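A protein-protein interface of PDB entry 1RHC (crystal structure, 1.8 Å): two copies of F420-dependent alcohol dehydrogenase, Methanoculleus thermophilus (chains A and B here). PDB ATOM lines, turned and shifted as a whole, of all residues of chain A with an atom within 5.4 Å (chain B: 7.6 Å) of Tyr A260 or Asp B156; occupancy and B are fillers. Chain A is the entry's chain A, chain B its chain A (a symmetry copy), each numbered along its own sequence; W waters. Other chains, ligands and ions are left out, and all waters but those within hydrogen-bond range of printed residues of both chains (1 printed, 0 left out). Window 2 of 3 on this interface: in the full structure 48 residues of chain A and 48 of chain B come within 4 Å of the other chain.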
ATOM      1  N   HIS A  41      26.151 -22.553 -13.844  1.00  0.00           N
ATOM      2  CA  HIS A  41      25.243 -22.742 -15.003  1.00  0.00           C
ATOM      3  C   HIS A  41      25.865 -23.769 -15.952  1.00  0.00           C
ATOM      4  O   HIS A  41      27.089 -23.812 -16.117  1.00  0.00           O
ATOM      5  CB  HIS A  41      25.007 -21.450 -15.816  1.00  0.00           C
ATOM      6  CG  HIS A  41      23.890 -20.589 -15.309  1.00  0.00           C
ATOM      7  ND1 HIS A  41      23.621 -19.345 -15.848  1.00  0.00           N
ATOM      8  CD2 HIS A  41      22.986 -20.770 -14.313  1.00  0.00           C
ATOM      9  CE1 HIS A  41      22.602 -18.801 -15.206  1.00  0.00           C
ATOM     10  NE2 HIS A  41      22.197 -19.642 -14.270  1.00  0.00           N
ATOM     11  N   ALA A 109      32.219 -17.319 -18.115  1.00  0.00           N
ATOM     12  CA  ALA A 109      31.215 -16.340 -17.727  1.00  0.00           C
ATOM     13  C   ALA A 109      29.928 -16.973 -17.221  1.00  0.00           C
ATOM     14  O   ALA A 109      29.270 -16.414 -16.341  1.00  0.00           O
ATOM     15  CB  ALA A 109      30.895 -15.356 -18.917  1.00  0.00           C
ATOM     16  N   MET A 110      29.588 -18.144 -17.759  1.00  0.00           N
ATOM     17  CA  MET A 110      28.343 -18.809 -17.383  1.00  0.00           C
ATOM     18  C   MET A 110      28.253 -19.167 -15.891  1.00  0.00           C
ATOM     19  O   MET A 110      27.156 -19.300 -15.358  1.00  0.00           O
ATOM     20  CB  MET A 110      28.138 -20.064 -18.226  1.00  0.00           C
ATOM     21  CG  MET A 110      29.053 -21.257 -17.874  1.00  0.00           C
ATOM     22  SD  MET A 110      28.745 -22.634 -19.016  1.00  0.00           S
ATOM     23  CE  MET A 110      29.618 -22.043 -20.470  1.00  0.00           C
ATOM     24  N   VAL A 113      29.288 -14.847 -13.882  1.00  0.00           N
ATOM     25  CA  VAL A 113      28.413 -13.695 -14.040  1.00  0.00           C
ATOM     26  C   VAL A 113      27.054 -13.759 -13.371  1.00  0.00           C
ATOM     27  O   VAL A 113      26.638 -12.796 -12.717  1.00  0.00           O
ATOM     28  CB  VAL A 113      28.201 -13.365 -15.550  1.00  0.00           C
ATOM     29  CG1 VAL A 113      27.231 -12.186 -15.670  1.00  0.00           C
ATOM     30  CG2 VAL A 113      29.549 -13.030 -16.189  1.00  0.00           C
ATOM     31  N   PRO A 114      26.346 -14.886 -13.493  1.00  0.00           N
ATOM     32  CA  PRO A 114      25.024 -14.943 -12.866  1.00  0.00           C
ATOM     33  C   PRO A 114      24.960 -14.611 -11.387  1.00  0.00           C
ATOM     34  O   PRO A 114      23.925 -14.174 -10.906  1.00  0.00           O
ATOM     35  CB  PRO A 114      24.550 -16.380 -13.127  1.00  0.00           C
ATOM     36  CG  PRO A 114      25.346 -16.809 -14.322  1.00  0.00           C
ATOM     37  CD  PRO A 114      26.700 -16.184 -14.104  1.00  0.00           C
ATOM     38  N   VAL A 115      26.061 -14.795 -10.666  1.00  0.00           N
ATOM     39  CA  VAL A 115      26.016 -14.548  -9.237  1.00  0.00           C
ATOM     40  C   VAL A 115      26.884 -13.417  -8.754  1.00  0.00           C
ATOM     41  O   VAL A 115      27.004 -13.213  -7.545  1.00  0.00           O
ATOM     42  CB  VAL A 115      26.370 -15.845  -8.433  1.00  0.00           C
ATOM     43  CG1 VAL A 115      25.462 -16.987  -8.890  1.00  0.00           C
ATOM     44  CG2 VAL A 115      27.837 -16.218  -8.643  1.00  0.00           C
ATOM     45  N   GLY A 117      27.580 -10.576 -11.478  1.00  0.00           N
ATOM     46  CA  GLY A 117      27.313  -9.487 -12.406  1.00  0.00           C
ATOM     47  C   GLY A 117      28.583  -8.911 -13.021  1.00  0.00           C
ATOM     48  O   GLY A 117      28.522  -7.934 -13.764  1.00  0.00           O
ATOM     49  N   LYS A 258      31.251 -12.480 -22.508  1.00  0.00           N
ATOM     50  CA  LYS A 258      30.296 -12.427 -21.419  1.00  0.00           C
ATOM     51  C   LYS A 258      28.978 -13.051 -21.863  1.00  0.00           C
ATOM     52  O   LYS A 258      27.975 -12.372 -22.058  1.00  0.00           O
ATOM     53  CB  LYS A 258      30.118 -10.971 -20.968  1.00  0.00           C
ATOM     54  CG  LYS A 258      29.329 -10.799 -19.676  1.00  0.00           C
ATOM     55  CD  LYS A 258      29.267  -9.330 -19.283  1.00  0.00           C
ATOM     56  CE  LYS A 258      28.831  -9.185 -17.843  1.00  0.00           C
ATOM     57  NZ  LYS A 258      28.561  -7.759 -17.532  1.00  0.00           N
ATOM     58  N   VAL A 259      29.000 -14.370 -22.009  1.00  0.00           N
ATOM     59  CA  VAL A 259      27.835 -15.148 -22.417  1.00  0.00           C
ATOM     60  C   VAL A 259      27.574 -16.105 -21.255  1.00  0.00           C
ATOM     61  O   VAL A 259      28.410 -16.955 -20.949  1.00  0.00           O
ATOM     62  CB  VAL A 259      28.149 -15.931 -23.698  1.00  0.00           C
ATOM     63  CG1 VAL A 259      26.954 -16.815 -24.069  1.00  0.00           C
ATOM     64  CG2 VAL A 259      28.442 -14.953 -24.837  1.00  0.00           C
ATOM     65  N   TYR A 260      26.413 -15.967 -20.624  1.00  0.00           N
ATOM     66  CA  TYR A 260      26.124 -16.745 -19.420  1.00  0.00           C
ATOM     67  C   TYR A 260      24.744 -17.371 -19.345  1.00  0.00           C
ATOM     68  O   TYR A 260      24.419 -18.030 -18.364  1.00  0.00           O
ATOM     69  CB  TYR A 260      26.378 -15.836 -18.209  1.00  0.00           C
ATOM     70  CG  TYR A 260      25.639 -14.501 -18.284  1.00  0.00           C
ATOM     71  CD1 TYR A 260      24.453 -14.316 -17.592  1.00  0.00           C
ATOM     72  CD2 TYR A 260      26.133 -13.436 -19.052  1.00  0.00           C
ATOM     73  CE1 TYR A 260      23.767 -13.109 -17.640  1.00  0.00           C
ATOM     74  CE2 TYR A 260      25.441 -12.203 -19.114  1.00  0.00           C
ATOM     75  CZ  TYR A 260      24.258 -12.063 -18.396  1.00  0.00           C
ATOM     76  OH  TYR A 260      23.539 -10.887 -18.410  1.00  0.00           O
ATOM     77  N   ASP A 261      23.927 -17.162 -20.378  1.00  0.00           N
ATOM     78  CA  ASP A 261      22.589 -17.738 -20.456  1.00  0.00           C
ATOM     79  C   ASP A 261      22.781 -19.060 -21.209  1.00  0.00           C
ATOM     80  O   ASP A 261      23.197 -19.046 -22.370  1.00  0.00           O
ATOM     81  CB  ASP A 261      21.685 -16.788 -21.260  1.00  0.00           C
ATOM     82  CG  ASP A 261      20.273 -17.328 -21.455  1.00  0.00           C
ATOM     83  OD1 ASP A 261      20.073 -18.547 -21.349  1.00  0.00           O
ATOM     84  OD2 ASP A 261      19.361 -16.517 -21.736  1.00  0.00           O
ATOM     85  N   PRO A 262      22.539 -20.224 -20.550  1.00  0.00           N
ATOM     86  CA  PRO A 262      22.707 -21.519 -21.219  1.00  0.00           C
ATOM     87  C   PRO A 262      21.904 -21.652 -22.540  1.00  0.00           C
ATOM     88  O   PRO A 262      22.267 -22.449 -23.397  1.00  0.00           O
ATOM     89  CB  PRO A 262      22.216 -22.527 -20.172  1.00  0.00           C
ATOM     90  CG  PRO A 262      22.598 -21.844 -18.852  1.00  0.00           C
ATOM     91  CD  PRO A 262      22.149 -20.412 -19.131  1.00  0.00           C
ATOM     92  N   GLU A 264      21.563 -19.321 -24.741  1.00  0.00           N
ATOM     93  CA  GLU A 264      22.357 -18.795 -25.839  1.00  0.00           C
ATOM     94  C   GLU A 264      23.639 -19.600 -26.024  1.00  0.00           C
ATOM     95  O   GLU A 264      24.142 -19.711 -27.133  1.00  0.00           O
ATOM     96  CB  GLU A 264      22.554 -17.271 -25.729  1.00  0.00           C
ATOM     97  CG  GLU A 264      23.731 -16.704 -25.032  1.00  0.00           C
ATOM     98  CD  GLU A 264      23.777 -15.187 -25.241  1.00  0.00           C
ATOM     99  OE1 GLU A 264      24.236 -14.716 -26.312  1.00  0.00           O
ATOM    100  OE2 GLU A 264      23.323 -14.459 -24.337  1.00  0.00           O
ATOM    101  N   VAL A 265      24.143 -20.241 -24.965  1.00  0.00           N
ATOM    102  CA  VAL A 265      25.315 -21.088 -25.150  1.00  0.00           C
ATOM    103  C   VAL A 265      24.910 -22.277 -26.021  1.00  0.00           C
ATOM    104  O   VAL A 265      25.663 -22.734 -26.894  1.00  0.00           O
ATOM    105  CB  VAL A 265      25.882 -21.610 -23.791  1.00  0.00           C
ATOM    106  CG1 VAL A 265      27.075 -22.536 -24.033  1.00  0.00           C
ATOM    107  CG2 VAL A 265      26.331 -20.444 -22.948  1.00  0.00           C
ATOM    108  N   PRO B 145      14.767 -17.858 -14.922  1.00  0.00           N
ATOM    109  CA  PRO B 145      15.950 -17.130 -14.458  1.00  0.00           C
ATOM    110  C   PRO B 145      15.544 -15.839 -13.789  1.00  0.00           C
ATOM    111  O   PRO B 145      14.564 -15.185 -14.181  1.00  0.00           O
ATOM    112  CB  PRO B 145      16.749 -16.894 -15.747  1.00  0.00           C
ATOM    113  CG  PRO B 145      16.363 -18.037 -16.602  1.00  0.00           C
ATOM    114  CD  PRO B 145      14.865 -18.141 -16.365  1.00  0.00           C
ATOM    115  N   VAL B 146      16.280 -15.465 -12.759  1.00  0.00           N
ATOM    116  CA  VAL B 146      15.947 -14.240 -12.064  1.00  0.00           C
ATOM    117  C   VAL B 146      17.084 -13.254 -12.122  1.00  0.00           C
ATOM    118  O   VAL B 146      18.248 -13.639 -12.077  1.00  0.00           O
ATOM    119  CB  VAL B 146      15.611 -14.500 -10.597  1.00  0.00           C
ATOM    120  CG1 VAL B 146      14.352 -15.331 -10.502  1.00  0.00           C
ATOM    121  CG2 VAL B 146      16.766 -15.198  -9.921  1.00  0.00           C
ATOM    122  N   THR B 147      16.738 -11.972 -12.241  1.00  0.00           N
ATOM    123  CA  THR B 147      17.733 -10.902 -12.260  1.00  0.00           C
ATOM    124  C   THR B 147      17.402 -10.024 -11.064  1.00  0.00           C
ATOM    125  O   THR B 147      16.239  -9.654 -10.853  1.00  0.00           O
ATOM    126  CB  THR B 147      17.650 -10.095 -13.563  1.00  0.00           C
ATOM    127  OG1 THR B 147      18.160 -10.902 -14.622  1.00  0.00           O
ATOM    128  CG2 THR B 147      18.460  -8.808 -13.460  1.00  0.00           C
ATOM    129  N   PHE B 148      18.414  -9.709 -10.270  1.00  0.00           N
ATOM    130  CA  PHE B 148      18.178  -8.972  -9.041  1.00  0.00           C
ATOM    131  C   PHE B 148      19.376  -8.151  -8.679  1.00  0.00           C
ATOM    132  O   PHE B 148      20.494  -8.654  -8.649  1.00  0.00           O
ATOM    133  CB  PHE B 148      17.861  -9.971  -7.909  1.00  0.00           C
ATOM    134  CG  PHE B 148      17.781  -9.342  -6.535  1.00  0.00           C
ATOM    135  CD1 PHE B 148      18.812  -9.515  -5.612  1.00  0.00           C
ATOM    136  CD2 PHE B 148      16.668  -8.606  -6.159  1.00  0.00           C
ATOM    137  CE1 PHE B 148      18.736  -8.975  -4.329  1.00  0.00           C
ATOM    138  CE2 PHE B 148      16.575  -8.052  -4.865  1.00  0.00           C
ATOM    139  CZ  PHE B 148      17.608  -8.240  -3.951  1.00  0.00           C
ATOM    140  N   LYS B 149      19.147  -6.873  -8.401  1.00  0.00           N
ATOM    141  CA  LYS B 149      20.236  -5.996  -8.036  1.00  0.00           C
ATOM    142  C   LYS B 149      19.915  -5.470  -6.655  1.00  0.00           C
ATOM    143  O   LYS B 149      19.160  -4.509  -6.499  1.00  0.00           O
ATOM    144  CB  LYS B 149      20.351  -4.843  -9.043  1.00  0.00           C
ATOM    145  CG  LYS B 149      21.486  -3.863  -8.737  1.00  0.00           C
ATOM    146  CD  LYS B 149      22.863  -4.543  -8.731  1.00  0.00           C
ATOM    147  CE  LYS B 149      23.391  -4.766 -10.149  1.00  0.00           C
ATOM    148  NZ  LYS B 149      22.419  -5.497 -11.024  1.00  0.00           N
ATOM    149  N   THR B 154      24.033  -9.574  -6.185  1.00  0.00           N
ATOM    150  CA  THR B 154      23.554  -9.496  -7.563  1.00  0.00           C
ATOM    151  C   THR B 154      23.212 -10.856  -8.156  1.00  0.00           C
ATOM    152  O   THR B 154      23.943 -11.825  -7.943  1.00  0.00           O
ATOM    153  CB  THR B 154      24.648  -8.896  -8.460  1.00  0.00           C
ATOM    154  OG1 THR B 154      24.986  -7.588  -7.978  1.00  0.00           O
ATOM    155  CG2 THR B 154      24.180  -8.812  -9.925  1.00  0.00           C
ATOM    156  N   LEU B 155      22.083 -10.945  -8.855  1.00  0.00           N
ATOM    157  CA  LEU B 155      21.752 -12.141  -9.628  1.00  0.00           C
ATOM    158  C   LEU B 155      21.533 -11.621 -11.059  1.00  0.00           C
ATOM    159  O   LEU B 155      20.868 -10.611 -11.254  1.00  0.00           O
ATOM    160  CB  LEU B 155      20.481 -12.840  -9.139  1.00  0.00           C
ATOM    161  CG  LEU B 155      20.562 -13.487  -7.740  1.00  0.00           C
ATOM    162  CD1 LEU B 155      19.235 -14.163  -7.402  1.00  0.00           C
ATOM    163  CD2 LEU B 155      21.720 -14.503  -7.719  1.00  0.00           C
ATOM    164  N   ASP B 156      22.098 -12.311 -12.044  1.00  0.00           N
ATOM    165  CA  ASP B 156      22.008 -11.874 -13.454  1.00  0.00           C
ATOM    166  C   ASP B 156      21.570 -13.082 -14.267  1.00  0.00           C
ATOM    167  O   ASP B 156      22.401 -13.921 -14.600  1.00  0.00           O
ATOM    168  CB  ASP B 156      23.392 -11.424 -13.907  1.00  0.00           C
ATOM    169  CG  ASP B 156      23.351 -10.435 -15.030  1.00  0.00           C
ATOM    170  OD1 ASP B 156      22.333 -10.394 -15.752  1.00  0.00           O
ATOM    171  OD2 ASP B 156      24.366  -9.720 -15.191  1.00  0.00           O
ATOM    172  N   LYS B 157      20.268 -13.172 -14.552  1.00  0.00           N
ATOM    173  CA  LYS B 157      19.688 -14.300 -15.281  1.00  0.00           C
ATOM    174  C   LYS B 157      20.074 -15.639 -14.613  1.00  0.00           C
ATOM    175  O   LYS B 157      20.311 -16.631 -15.295  1.00  0.00           O
ATOM    176  CB  LYS B 157      20.171 -14.301 -16.734  1.00  0.00           C
ATOM    177  CG  LYS B 157      19.895 -12.958 -17.418  1.00  0.00           C
ATOM    178  CD  LYS B 157      20.025 -13.056 -18.922  1.00  0.00           C
ATOM    179  CE  LYS B 157      19.788 -11.680 -19.528  1.00  0.00           C
ATOM    180  NZ  LYS B 157      19.764 -11.778 -21.012  1.00  0.00           N
ATOM    181  N   ALA B 158      20.083 -15.655 -13.281  1.00  0.00           N
ATOM    182  CA  ALA B 158      20.493 -16.845 -12.518  1.00  0.00           C
ATOM    183  C   ALA B 158      19.373 -17.849 -12.368  1.00  0.00           C
ATOM    184  O   ALA B 158      18.223 -17.478 -12.110  1.00  0.00           O
ATOM    185  CB  ALA B 158      20.974 -16.419 -11.137  1.00  0.00           C
ATOM    186  N   PHE B 159      19.710 -19.131 -12.504  1.00  0.00           N
ATOM    187  CA  PHE B 159      18.708 -20.185 -12.379  1.00  0.00           C
ATOM    188  C   PHE B 159      19.335 -21.423 -11.731  1.00  0.00           C
ATOM    189  O   PHE B 159      20.483 -21.775 -12.049  1.00  0.00           O
ATOM    190  CB  PHE B 159      18.184 -20.575 -13.766  1.00  0.00           C
ATOM    191  CG  PHE B 159      17.054 -21.574 -13.733  1.00  0.00           C
ATOM    192  CD1 PHE B 159      15.783 -21.202 -13.270  1.00  0.00           C
ATOM    193  CD2 PHE B 159      17.253 -22.888 -14.156  1.00  0.00           C
ATOM    194  CE1 PHE B 159      14.711 -22.128 -13.228  1.00  0.00           C
ATOM    195  CE2 PHE B 159      16.190 -23.825 -14.122  1.00  0.00           C
ATOM    196  CZ  PHE B 159      14.912 -23.435 -13.651  1.00  0.00           C
ATOM    197  N   TYR B 161      19.510 -25.074 -11.828  1.00  0.00           N
ATOM    198  CA  TYR B 161      19.152 -26.231 -12.634  1.00  0.00           C
ATOM    199  C   TYR B 161      18.978 -27.496 -11.803  1.00  0.00           C
ATOM    200  O   TYR B 161      18.281 -28.407 -12.217  1.00  0.00           O
ATOM    201  CB  TYR B 161      20.202 -26.463 -13.714  1.00  0.00           C
ATOM    202  CG  TYR B 161      20.079 -25.453 -14.821  1.00  0.00           C
ATOM    203  CD1 TYR B 161      20.660 -24.186 -14.714  1.00  0.00           C
ATOM    204  CD2 TYR B 161      19.316 -25.748 -15.960  1.00  0.00           C
ATOM    205  CE1 TYR B 161      20.477 -23.217 -15.738  1.00  0.00           C
ATOM    206  CE2 TYR B 161      19.134 -24.808 -16.957  1.00  0.00           C
ATOM    207  CZ  TYR B 161      19.707 -23.560 -16.844  1.00  0.00           C
ATOM    208  OH  TYR B 161      19.497 -22.669 -17.867  1.00  0.00           O
HETATM  209  O   HOH W   1      26.360 -11.125  -5.486  1.00  0.00           O
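His A41 touches Lys B157.
Ala B158 touches His A41 (CA to NE2, 3.7 Å).
His A41 touches Tyr B161 (CD2 to CE1, 3.8 Å).
O of Val A113 touches CB of Asp B156, at 3.7 Å.
O of Pro A114 touches O of Thr B154, 3.8 Å away.
Pro A114 touches Leu B155.
CB of Ala B158 touches O of Pro A114, 3.7 Å away.
Lys B157 touches Tyr A260.
CG of Pro A262 touches OH of Tyr B161, at 3.4 Å.
Of the 12 printed residues of chain B, 7 touch a printed residue of chain A.
Hydrophobic or aromatic side chains of chain B within 4 Å of the printed part of chain A: Leu B155, Ala B158 and Tyr B161.
Among the printed residues, no Asp or Glu carboxylate lies within 4 Å of a Lys or Arg side-chain nitrogen of the other chain.
Water W1 lies within hydrogen-bond range of N of Thr B154 (2.9 Å) and O of Val A115 (3.0 Å).
A ring nitrogen (NE2) of His A41 lies within hydrogen-bond range of the backbone NH (N) of Phe B159 (3.1 Å).
N of Asp B156 lies within hydrogen-bond range of O of Pro A114 (2.8 Å).
The side-chain hydroxyl (OH) of Tyr A260 lies within hydrogen-bond range of the side-chain carboxylate (OD1) of Asp B156 (3.0 Å).
O of Val A115 lies close to O of Thr B154 (3.4 Å).
The backbone carbonyl oxygen (O) of Tyr A260 lies within hydrogen-bond range of a ring nitrogen (ND1) of His A41, at 2.9 Å.
The backbone NH (N) of Lys B157 lies within hydrogen-bond range of the backbone carbonyl oxygen (O) of Val B146.
N of Val B146 sits at hydrogen-bond distance from O of Ala B158, 2.9 Å away.
The backbone NH of Lys B157 lies within hydrogen-bond range of the side-chain hydroxyl of Thr B147 (3.1 Å).
The backbone NH of Phe B148 sits at hydrogen-bond distance from the backbone carbonyl oxygen of Leu B155 (2.8 Å).
No position is printed for both chains.
Of chain B, only Asp B156 and Lys B157 come within 4 Å of Tyr A260.
Of chain A, only Val A113 (3.7 Å), Pro A114 (2.8 Å) and Tyr A260 (3.0 Å) come within 4 Å of Asp B156.
Of the printed residues of chain A, Lys B157 touches His A41 (3.2 Å) and Tyr A260 (3.9 Å).
Of the printed residues of chain B, Pro A114 touches Thr B154 (3.8 Å), Leu B155 (3.2 Å), Asp B156 (2.8 Å) and Ala B158 (3.7 Å).
Printed residues of chain A within 4 Å of Phe B159: His A41.
Printed residues of chain B within 4 Å of Val A115: Thr B154 (3.4 Å).
Lys A258 touches none of the printed residues of chain B.
The nearest residue of chain A that does not touch Asp B156 is Gly A117 (4.1 Å).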
